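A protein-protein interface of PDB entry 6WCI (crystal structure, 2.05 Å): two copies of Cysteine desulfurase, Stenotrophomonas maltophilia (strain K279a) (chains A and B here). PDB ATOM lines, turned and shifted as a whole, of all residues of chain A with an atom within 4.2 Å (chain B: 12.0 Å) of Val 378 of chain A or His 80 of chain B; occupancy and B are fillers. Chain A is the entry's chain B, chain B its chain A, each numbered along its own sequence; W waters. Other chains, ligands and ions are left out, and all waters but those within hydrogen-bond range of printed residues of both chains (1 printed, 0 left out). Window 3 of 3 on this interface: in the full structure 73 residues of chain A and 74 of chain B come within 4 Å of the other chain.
A ring nitrogen (NE2) of His 80 of chain B sits at hydrogen-bond distance from the side-chain carboxylate of Asp 49 of chain A (3.0 Å). The side-chain carboxylate (OD1) of Asp 372 of chain A is in hydrogen-bond range of the backbone NH (N) of Ala 81 of chain B.
His 80 of chain B touches Asp 372 of chain A (CB to OD1, 3.4 Å). Ala 377 of chain A touches His 80 of chain B. O of Val 378 of chain A touches CD2 of His 80 of chain B, at 3.1 Å.
Val 378 of chain A touches just one residue of chain B: His 80 (3.1 Å). Printed residues of chain A within 4 Å of His 80 of chain B: Asp 49 (3.0 Å), Asp 372 (3.4 Å), Ala 377 (3.7 Å) and Val 378 (3.1 Å). No residue of chain B comes within 4 Å of Phe 48 of chain A. No residue of chain B comes within 4 Å of Ala 368 of chain A. No residue of chain B comes within 4 Å of Leu 371 of chain A. Of chain B, only His 80 (3.4 Å) and Ala 81 (2.9 Å) come within 4 Å of Asp 372 of chain A. No residue of chain B comes within 4 Å of Val 376 of chain A. Ala 377 of chain A touches just one residue of chain B: His 80 (3.7 Å). Of the printed residues of chain A, Ala 81 of chain B touches Asp 372 (2.9 Å). The nearest residue of chain B that does not touch Val 378 of chain A is Val 79 of chain B (5.9 Å).
No position is printed for both chains.
Of the 19 printed residues of chain B, 2 touch a printed residue of chain A. Hydrophobic or aromatic side chains of chain B that line the printed part of chain A: His 80 and Ala 81. Hydrophobic or aromatic side chains of chain A that line the printed part of chain B: Ala 377.
Water W1 bridges the side-chain carboxylate (OD2) of Asp 49 of chain A (2.9 Å) and the backbone NH (N) of Asn 74 of chain B (3.3 Å).
The backbone NH (N) of Gly 83 of chain B lies within hydrogen-bond range of a ring nitrogen (ND1) of His 80 of chain B (3.1 Å). The backbone NH (N) of Phe 48 of chain A is in hydrogen-bond range of the backbone carbonyl oxygen (O) of Ala 377 of chain A (2.8 Å). The backbone carbonyl oxygen (O) of Ala 377 of chain A is in hydrogen-bond range of the backbone NH (N) of Asp 49 of chain A (3.3 Å). OD1 of Asp 49 of chain A is in salt-bridge range of NH2 of Arg 399 of chain A (3.4 Å).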
ATOM      1  N   PHE A  48      22.259   1.701  -7.612  1.00  0.00           N
ATOM      2  CA  PHE A  48      20.952   2.018  -7.042  1.00  0.00           C
ATOM      3  C   PHE A  48      21.119   2.873  -5.790  1.00  0.00           C
ATOM      4  O   PHE A  48      20.365   2.740  -4.824  1.00  0.00           O
ATOM      5  CB  PHE A  48      20.158   0.749  -6.731  1.00  0.00           C
ATOM      6  CG  PHE A  48      19.511   0.094  -7.950  1.00  0.00           C
ATOM      7  CD1 PHE A  48      19.690   0.605  -9.229  1.00  0.00           C
ATOM      8  CD2 PHE A  48      18.716  -1.030  -7.798  1.00  0.00           C
ATOM      9  CE1 PHE A  48      19.087  -0.007 -10.331  1.00  0.00           C
ATOM     10  CE2 PHE A  48      18.110  -1.642  -8.889  1.00  0.00           C
ATOM     11  CZ  PHE A  48      18.296  -1.131 -10.155  1.00  0.00           C
ATOM     12  N   ASP A  49      22.126   3.756  -5.792  1.00  0.00           N
ATOM     13  CA  ASP A  49      22.380   4.662  -4.674  1.00  0.00           C
ATOM     14  C   ASP A  49      22.352   6.120  -5.133  1.00  0.00           C
ATOM     15  O   ASP A  49      23.144   6.951  -4.684  1.00  0.00           O
ATOM     16  CB  ASP A  49      23.712   4.337  -3.997  1.00  0.00           C
ATOM     17  CG  ASP A  49      23.809   4.919  -2.601  1.00  0.00           C
ATOM     18  OD1 ASP A  49      22.748   5.150  -1.996  1.00  0.00           O
ATOM     19  OD2 ASP A  49      24.940   5.174  -2.117  1.00  0.00           O
ATOM     20  N   ALA A 368      23.322  -4.744   2.208  1.00  0.00           N
ATOM     21  CA  ALA A 368      24.157  -3.889   1.367  1.00  0.00           C
ATOM     22  C   ALA A 368      25.507  -4.539   1.089  1.00  0.00           C
ATOM     23  O   ALA A 368      25.974  -4.543  -0.055  1.00  0.00           O
ATOM     24  CB  ALA A 368      24.351  -2.514   2.018  1.00  0.00           C
ATOM     25  N   LEU A 371      25.006  -7.348  -1.381  1.00  0.00           N
ATOM     26  CA  LEU A 371      24.534  -6.877  -2.677  1.00  0.00           C
ATOM     27  C   LEU A 371      25.681  -6.270  -3.474  1.00  0.00           C
ATOM     28  O   LEU A 371      25.785  -6.485  -4.689  1.00  0.00           O
ATOM     29  CB  LEU A 371      23.393  -5.874  -2.507  1.00  0.00           C
ATOM     30  CG  LEU A 371      22.009  -6.449  -2.205  1.00  0.00           C
ATOM     31  CD1 LEU A 371      20.997  -5.350  -1.932  1.00  0.00           C
ATOM     32  CD2 LEU A 371      21.538  -7.350  -3.345  1.00  0.00           C
ATOM     33  N   ASP A 372      26.577  -5.542  -2.796  1.00  0.00           N
ATOM     34  CA  ASP A 372      27.750  -4.986  -3.468  1.00  0.00           C
ATOM     35  C   ASP A 372      28.604  -6.079  -4.093  1.00  0.00           C
ATOM     36  O   ASP A 372      29.152  -5.899  -5.186  1.00  0.00           O
ATOM     37  CB  ASP A 372      28.585  -4.163  -2.494  1.00  0.00           C
ATOM     38  CG  ASP A 372      29.910  -3.735  -3.094  1.00  0.00           C
ATOM     39  OD1 ASP A 372      29.911  -2.832  -3.964  1.00  0.00           O
ATOM     40  OD2 ASP A 372      30.944  -4.321  -2.709  1.00  0.00           O
ATOM     41  N   VAL A 376      25.780  -4.661  -7.018  1.00  0.00           N
ATOM     42  CA  VAL A 376      24.670  -3.762  -6.740  1.00  0.00           C
ATOM     43  C   VAL A 376      25.095  -2.774  -5.665  1.00  0.00           C
ATOM     44  O   VAL A 376      25.535  -3.170  -4.581  1.00  0.00           O
ATOM     45  CB  VAL A 376      23.419  -4.539  -6.295  1.00  0.00           C
ATOM     46  CG1 VAL A 376      22.317  -3.557  -5.933  1.00  0.00           C
ATOM     47  CG2 VAL A 376      22.953  -5.488  -7.380  1.00  0.00           C
ATOM     48  N   ALA A 377      24.956  -1.490  -5.956  1.00  0.00           N
ATOM     49  CA  ALA A 377      25.271  -0.442  -4.995  1.00  0.00           C
ATOM     50  C   ALA A 377      23.969   0.093  -4.410  1.00  0.00           C
ATOM     51  O   ALA A 377      23.162   0.703  -5.116  1.00  0.00           O
ATOM     52  CB  ALA A 377      26.082   0.674  -5.648  1.00  0.00           C
ATOM     53  N   VAL A 378      23.753  -0.163  -3.127  1.00  0.00           N
ATOM     54  CA  VAL A 378      22.698   0.477  -2.358  1.00  0.00           C
ATOM     55  C   VAL A 378      23.313   0.985  -1.062  1.00  0.00           C
ATOM     56  O   VAL A 378      24.493   0.781  -0.788  1.00  0.00           O
ATOM     57  CB  VAL A 378      21.509  -0.469  -2.069  1.00  0.00           C
ATOM     58  CG1 VAL A 378      20.905  -0.989  -3.359  1.00  0.00           C
ATOM     59  CG2 VAL A 378      21.946  -1.618  -1.182  1.00  0.00           C
ATOM     60  N   ARG A 379      22.492   1.640  -0.257  1.00  0.00           N
ATOM     61  CA  ARG A 379      22.940   2.217   0.998  1.00  0.00           C
ATOM     62  C   ARG A 379      22.054   1.699   2.116  1.00  0.00           C
ATOM     63  O   ARG A 379      20.823   1.758   2.012  1.00  0.00           O
ATOM     64  CB  ARG A 379      22.878   3.738   0.940  1.00  0.00           C
ATOM     65  CG  ARG A 379      23.278   4.439   2.223  1.00  0.00           C
ATOM     66  CD  ARG A 379      24.691   4.062   2.631  1.00  0.00           C
ATOM     67  NE  ARG A 379      25.259   5.007   3.587  1.00  0.00           N
ATOM     68  CZ  ARG A 379      26.255   4.708   4.416  1.00  0.00           C
ATOM     69  NH1 ARG A 379      26.779   3.485   4.404  1.00  0.00           N
ATOM     70  NH2 ARG A 379      26.717   5.621   5.259  1.00  0.00           N
ATOM     71  N   CYS A 398      17.413  -0.667   4.234  1.00  0.00           N
ATOM     72  CA  CYS A 398      18.145  -0.773   2.983  1.00  0.00           C
ATOM     73  C   CYS A 398      17.431   0.086   1.952  1.00  0.00           C
ATOM     74  O   CYS A 398      16.206   0.019   1.826  1.00  0.00           O
ATOM     75  CB  CYS A 398      18.239  -2.221   2.512  1.00  0.00           C
ATOM     76  SG  CYS A 398      19.478  -2.459   1.219  1.00  0.00           S
ATOM     77  N   ARG A 399      18.185   0.919   1.241  1.00  0.00           N
ATOM     78  CA  ARG A 399      17.575   1.916   0.376  1.00  0.00           C
ATOM     79  C   ARG A 399      18.095   1.757  -1.037  1.00  0.00           C
ATOM     80  O   ARG A 399      19.296   1.910  -1.283  1.00  0.00           O
ATOM     81  CB  ARG A 399      17.834   3.332   0.877  1.00  0.00           C
ATOM     82  CG  ARG A 399      17.080   4.376   0.077  1.00  0.00           C
ATOM     83  CD  ARG A 399      17.536   5.791   0.423  1.00  0.00           C
ATOM     84  NE  ARG A 399      18.950   5.993   0.113  1.00  0.00           N
ATOM     85  CZ  ARG A 399      19.619   7.116   0.362  1.00  0.00           C
ATOM     86  NH1 ARG A 399      18.996   8.145   0.917  1.00  0.00           N
ATOM     87  NH2 ARG A 399      20.906   7.216   0.049  1.00  0.00           N
ATOM     88  N   PHE A 414      18.670  -6.883 -10.221  1.00  0.00           N
ATOM     89  CA  PHE A 414      18.681  -6.580  -8.794  1.00  0.00           C
ATOM     90  C   PHE A 414      17.912  -7.637  -8.003  1.00  0.00           C
ATOM     91  O   PHE A 414      18.401  -8.158  -6.994  1.00  0.00           O
ATOM     92  CB  PHE A 414      18.086  -5.187  -8.568  1.00  0.00           C
ATOM     93  CG  PHE A 414      17.896  -4.822  -7.119  1.00  0.00           C
ATOM     94  CD1 PHE A 414      16.764  -5.230  -6.421  1.00  0.00           C
ATOM     95  CD2 PHE A 414      18.839  -4.048  -6.462  1.00  0.00           C
ATOM     96  CE1 PHE A 414      16.594  -4.887  -5.094  1.00  0.00           C
ATOM     97  CE2 PHE A 414      18.675  -3.699  -5.137  1.00  0.00           C
ATOM     98  CZ  PHE A 414      17.554  -4.115  -4.451  1.00  0.00           C
ATOM     99  N   PHE B  67      37.517  10.686 -11.300  1.00  0.00           N
ATOM    100  CA  PHE B  67      36.520  10.498 -10.253  1.00  0.00           C
ATOM    101  C   PHE B  67      35.120  10.449 -10.852  1.00  0.00           C
ATOM    102  O   PHE B  67      34.357   9.512 -10.603  1.00  0.00           O
ATOM    103  CB  PHE B  67      36.634  11.610  -9.211  1.00  0.00           C
ATOM    104  CG  PHE B  67      35.547  11.586  -8.174  1.00  0.00           C
ATOM    105  CD1 PHE B  67      35.545  10.634  -7.176  1.00  0.00           C
ATOM    106  CD2 PHE B  67      34.527  12.530  -8.194  1.00  0.00           C
ATOM    107  CE1 PHE B  67      34.542  10.617  -6.208  1.00  0.00           C
ATOM    108  CE2 PHE B  67      33.522  12.521  -7.233  1.00  0.00           C
ATOM    109  CZ  PHE B  67      33.530  11.562  -6.237  1.00  0.00           C
ATOM    110  N   ARG B  70      34.803   7.167 -13.076  1.00  0.00           N
ATOM    111  CA  ARG B  70      35.068   5.802 -12.633  1.00  0.00           C
ATOM    112  C   ARG B  70      34.608   5.491 -11.207  1.00  0.00           C
ATOM    113  O   ARG B  70      34.217   4.355 -10.943  1.00  0.00           O
ATOM    114  CB  ARG B  70      36.560   5.478 -12.781  1.00  0.00           C
ATOM    115  CG  ARG B  70      36.884   3.976 -12.703  1.00  0.00           C
ATOM    116  CD  ARG B  70      38.401   3.655 -12.850  1.00  0.00           C
ATOM    117  NE  ARG B  70      39.229   4.394 -11.891  1.00  0.00           N
ATOM    118  CZ  ARG B  70      39.195   4.210 -10.572  1.00  0.00           C
ATOM    119  NH1 ARG B  70      38.373   3.309 -10.031  1.00  0.00           N
ATOM    120  NH2 ARG B  70      39.980   4.927  -9.788  1.00  0.00           N
ATOM    121  N   TYR B  71      34.644   6.444 -10.260  1.00  0.00           N
ATOM    122  CA  TYR B  71      34.211   6.055  -8.918  1.00  0.00           C
ATOM    123  C   TYR B  71      33.425   7.148  -8.190  1.00  0.00           C
ATOM    124  O   TYR B  71      33.495   7.248  -6.956  1.00  0.00           O
ATOM    125  CB  TYR B  71      35.411   5.550  -8.083  1.00  0.00           C
ATOM    126  CG  TYR B  71      36.537   6.541  -7.843  1.00  0.00           C
ATOM    127  CD1 TYR B  71      37.435   6.867  -8.852  1.00  0.00           C
ATOM    128  CD2 TYR B  71      36.716   7.128  -6.593  1.00  0.00           C
ATOM    129  CE1 TYR B  71      38.477   7.766  -8.638  1.00  0.00           C
ATOM    130  CE2 TYR B  71      37.754   8.030  -6.361  1.00  0.00           C
ATOM    131  CZ  TYR B  71      38.631   8.349  -7.388  1.00  0.00           C
ATOM    132  OH  TYR B  71      39.660   9.247  -7.159  1.00  0.00           O
ATOM    133  N   ASN B  72      32.621   7.920  -8.921  1.00  0.00           N
ATOM    134  CA  ASN B  72      31.766   8.918  -8.280  1.00  0.00           C
ATOM    135  C   ASN B  72      30.757   8.269  -7.330  1.00  0.00           C
ATOM    136  O   ASN B  72      29.873   7.526  -7.761  1.00  0.00           O
ATOM    137  CB  ASN B  72      31.028   9.746  -9.334  1.00  0.00           C
ATOM    138  CG  ASN B  72      30.019  10.715  -8.715  1.00  0.00           C
ATOM    139  OD1 ASN B  72      30.398  11.719  -8.127  1.00  0.00           O
ATOM    140  ND2 ASN B  72      28.732  10.394  -8.830  1.00  0.00           N
ATOM    141  N   ALA B  73      30.889   8.573  -6.039  1.00  0.00           N
ATOM    142  CA  ALA B  73      29.974   8.120  -5.001  1.00  0.00           C
ATOM    143  C   ALA B  73      30.204   8.992  -3.779  1.00  0.00           C
ATOM    144  O   ALA B  73      31.225   9.678  -3.677  1.00  0.00           O
ATOM    145  CB  ALA B  73      30.183   6.643  -4.661  1.00  0.00           C
ATOM    146  N   ASN B  74      29.261   8.950  -2.841  1.00  0.00           N
ATOM    147  CA  ASN B  74      29.455   9.761  -1.648  1.00  0.00           C
ATOM    148  C   ASN B  74      30.421   9.057  -0.701  1.00  0.00           C
ATOM    149  O   ASN B  74      30.814   7.907  -0.915  1.00  0.00           O
ATOM    150  CB  ASN B  74      28.123  10.070  -0.963  1.00  0.00           C
ATOM    151  CG  ASN B  74      28.144  11.421  -0.203  1.00  0.00           C
ATOM    152  OD1 ASN B  74      29.189  11.868   0.271  1.00  0.00           O
ATOM    153  ND2 ASN B  74      26.990  12.061  -0.101  1.00  0.00           N
ATOM    154  N   VAL B  75      30.830   9.770   0.342  1.00  0.00           N
ATOM    155  CA  VAL B  75      31.901   9.300   1.207  1.00  0.00           C
ATOM    156  C   VAL B  75      31.378   9.032   2.613  1.00  0.00           C
ATOM    157  O   VAL B  75      30.236   9.361   2.925  1.00  0.00           O
ATOM    158  CB  VAL B  75      33.071  10.311   1.241  1.00  0.00           C
ATOM    159  CG1 VAL B  75      33.649  10.531  -0.165  1.00  0.00           C
ATOM    160  CG2 VAL B  75      32.629  11.625   1.843  1.00  0.00           C
ATOM    161  N   VAL B  79      30.455   1.249   3.285  1.00  0.00           N
ATOM    162  CA  VAL B  79      29.627   1.403   2.100  1.00  0.00           C
ATOM    163  C   VAL B  79      30.059   0.407   1.009  1.00  0.00           C
ATOM    164  O   VAL B  79      30.779  -0.549   1.280  1.00  0.00           O
ATOM    165  CB  VAL B  79      29.678   2.852   1.573  1.00  0.00           C
ATOM    166  N   HIS B  80      29.620   0.657  -0.223  1.00  0.00           N
ATOM    167  CA  HIS B  80      29.867  -0.215  -1.363  1.00  0.00           C
ATOM    168  C   HIS B  80      31.199   0.154  -2.038  1.00  0.00           C
ATOM    169  O   HIS B  80      31.936   1.030  -1.576  1.00  0.00           O
ATOM    170  CB  HIS B  80      28.674  -0.129  -2.314  1.00  0.00           C
ATOM    171  CG  HIS B  80      28.204   1.274  -2.549  1.00  0.00           C
ATOM    172  ND1 HIS B  80      29.006   2.234  -3.130  1.00  0.00           N
ATOM    173  CD2 HIS B  80      27.036   1.894  -2.250  1.00  0.00           C
ATOM    174  CE1 HIS B  80      28.349   3.379  -3.194  1.00  0.00           C
ATOM    175  NE2 HIS B  80      27.153   3.202  -2.664  1.00  0.00           N
ATOM    176  N   ALA B  81      31.503  -0.497  -3.164  1.00  0.00           N
ATOM    177  CA  ALA B  81      32.843  -0.408  -3.753  1.00  0.00           C
ATOM    178  C   ALA B  81      33.199   1.020  -4.151  1.00  0.00           C
ATOM    179  O   ALA B  81      34.273   1.519  -3.800  1.00  0.00           O
ATOM    180  CB  ALA B  81      32.959  -1.340  -4.961  1.00  0.00           C
ATOM    181  N   LEU B  82      32.323   1.689  -4.905  1.00  0.00           N
ATOM    182  CA  LEU B  82      32.633   3.055  -5.324  1.00  0.00           C
ATOM    183  C   LEU B  82      32.632   4.012  -4.134  1.00  0.00           C
ATOM    184  O   LEU B  82      33.480   4.906  -4.053  1.00  0.00           O
ATOM    185  CB  LEU B  82      31.643   3.536  -6.388  1.00  0.00           C
ATOM    186  CG  LEU B  82      31.876   3.199  -7.862  1.00  0.00           C
ATOM    187  CD1 LEU B  82      31.717   1.710  -8.117  1.00  0.00           C
ATOM    188  CD2 LEU B  82      30.909   4.011  -8.708  1.00  0.00           C
ATOM    189  N   GLY B  83      31.686   3.850  -3.207  1.00  0.00           N
ATOM    190  CA  GLY B  83      31.695   4.693  -2.019  1.00  0.00           C
ATOM    191  C   GLY B  83      32.945   4.495  -1.186  1.00  0.00           C
ATOM    192  O   GLY B  83      33.448   5.438  -0.568  1.00  0.00           O
ATOM    193  N   SER B  84      33.480   3.275  -1.192  1.00  0.00           N
ATOM    194  CA  SER B  84      34.674   2.943  -0.429  1.00  0.00           C
ATOM    195  C   SER B  84      35.908   3.618  -1.015  1.00  0.00           C
ATOM    196  O   SER B  84      36.732   4.173  -0.280  1.00  0.00           O
ATOM    197  CB  SER B  84      34.841   1.420  -0.412  1.00  0.00           C
ATOM    198  OG  SER B  84      35.743   0.989   0.585  1.00  0.00           O
ATOM    199  N   GLU B  85      36.066   3.562  -2.345  1.00  0.00           N
ATOM    200  CA  GLU B  85      37.204   4.223  -2.973  1.00  0.00           C
ATOM    201  C   GLU B  85      37.077   5.738  -2.903  1.00  0.00           C
ATOM    202  O   GLU B  85      38.090   6.441  -2.788  1.00  0.00           O
ATOM    203  CB  GLU B  85      37.353   3.774  -4.428  1.00  0.00           C
ATOM    204  CG  GLU B  85      38.629   4.297  -5.103  1.00  0.00           C
ATOM    205  CD  GLU B  85      38.837   3.754  -6.509  1.00  0.00           C
ATOM    206  OE1 GLU B  85      37.912   3.128  -7.067  1.00  0.00           O
ATOM    207  OE2 GLU B  85      39.939   3.946  -7.057  1.00  0.00           O
ATOM    208  N   ALA B  86      35.854   6.263  -2.980  1.00  0.00           N
ATOM    209  CA  ALA B  86      35.694   7.710  -2.911  1.00  0.00           C
ATOM    210  C   ALA B  86      36.110   8.227  -1.544  1.00  0.00           C
ATOM    211  O   ALA B  86      36.760   9.277  -1.438  1.00  0.00           O
ATOM    212  CB  ALA B  86      34.250   8.090  -3.220  1.00  0.00           C
ATOM    213  N   THR B  87      35.752   7.482  -0.490  1.00  0.00           N
ATOM    214  CA  THR B  87      36.083   7.864   0.878  1.00  0.00           C
ATOM    215  C   THR B  87      37.583   7.801   1.118  1.00  0.00           C
ATOM    216  O   THR B  87      38.166   8.731   1.691  1.00  0.00           O
ATOM    217  CB  THR B  87      35.356   6.953   1.867  1.00  0.00           C
ATOM    218  OG1 THR B  87      33.946   7.007   1.622  1.00  0.00           O
ATOM    219  CG2 THR B  87      35.638   7.380   3.294  1.00  0.00           C
ATOM    220  N   ASP B  88      38.226   6.713   0.684  1.00  0.00           N
ATOM    221  CA  ASP B  88      39.673   6.603   0.849  1.00  0.00           C
ATOM    222  C   ASP B  88      40.396   7.723   0.118  1.00  0.00           C
ATOM    223  O   ASP B  88      41.407   8.238   0.605  1.00  0.00           O
ATOM    224  CB  ASP B  88      40.171   5.247   0.358  1.00  0.00           C
ATOM    225  CG  ASP B  88      39.813   4.123   1.309  1.00  0.00           C
ATOM    226  OD1 ASP B  88      39.797   4.370   2.537  1.00  0.00           O
ATOM    227  OD2 ASP B  88      39.541   2.998   0.831  1.00  0.00           O
ATOM    228  N   ALA B  89      39.893   8.105  -1.056  1.00  0.00           N
ATOM    229  CA  ALA B  89      40.469   9.225  -1.790  1.00  0.00           C
ATOM    230  C   ALA B  89      40.261  10.532  -1.039  1.00  0.00           C
ATOM    231  O   ALA B  89      41.188  11.336  -0.906  1.00  0.00           O
ATOM    232  CB  ALA B  89      39.847   9.306  -3.183  1.00  0.00           C
ATOM    233  N   ILE B 300      33.663  16.561  -2.898  1.00  0.00           N
ATOM    234  CA  ILE B 300      34.490  15.355  -2.956  1.00  0.00           C
ATOM    235  C   ILE B 300      35.480  15.430  -4.117  1.00  0.00           C
ATOM    236  O   ILE B 300      36.677  15.172  -3.952  1.00  0.00           O
ATOM    237  CB  ILE B 300      33.623  14.094  -3.074  1.00  0.00           C
ATOM    238  CG1 ILE B 300      32.642  13.952  -1.896  1.00  0.00           C
ATOM    239  CG2 ILE B 300      34.536  12.894  -3.164  1.00  0.00           C
ATOM    240  CD1 ILE B 300      31.595  12.832  -2.126  1.00  0.00           C
HETATM  241  O   HOH W   1      26.921   6.785  -3.519  1.00  0.00           O
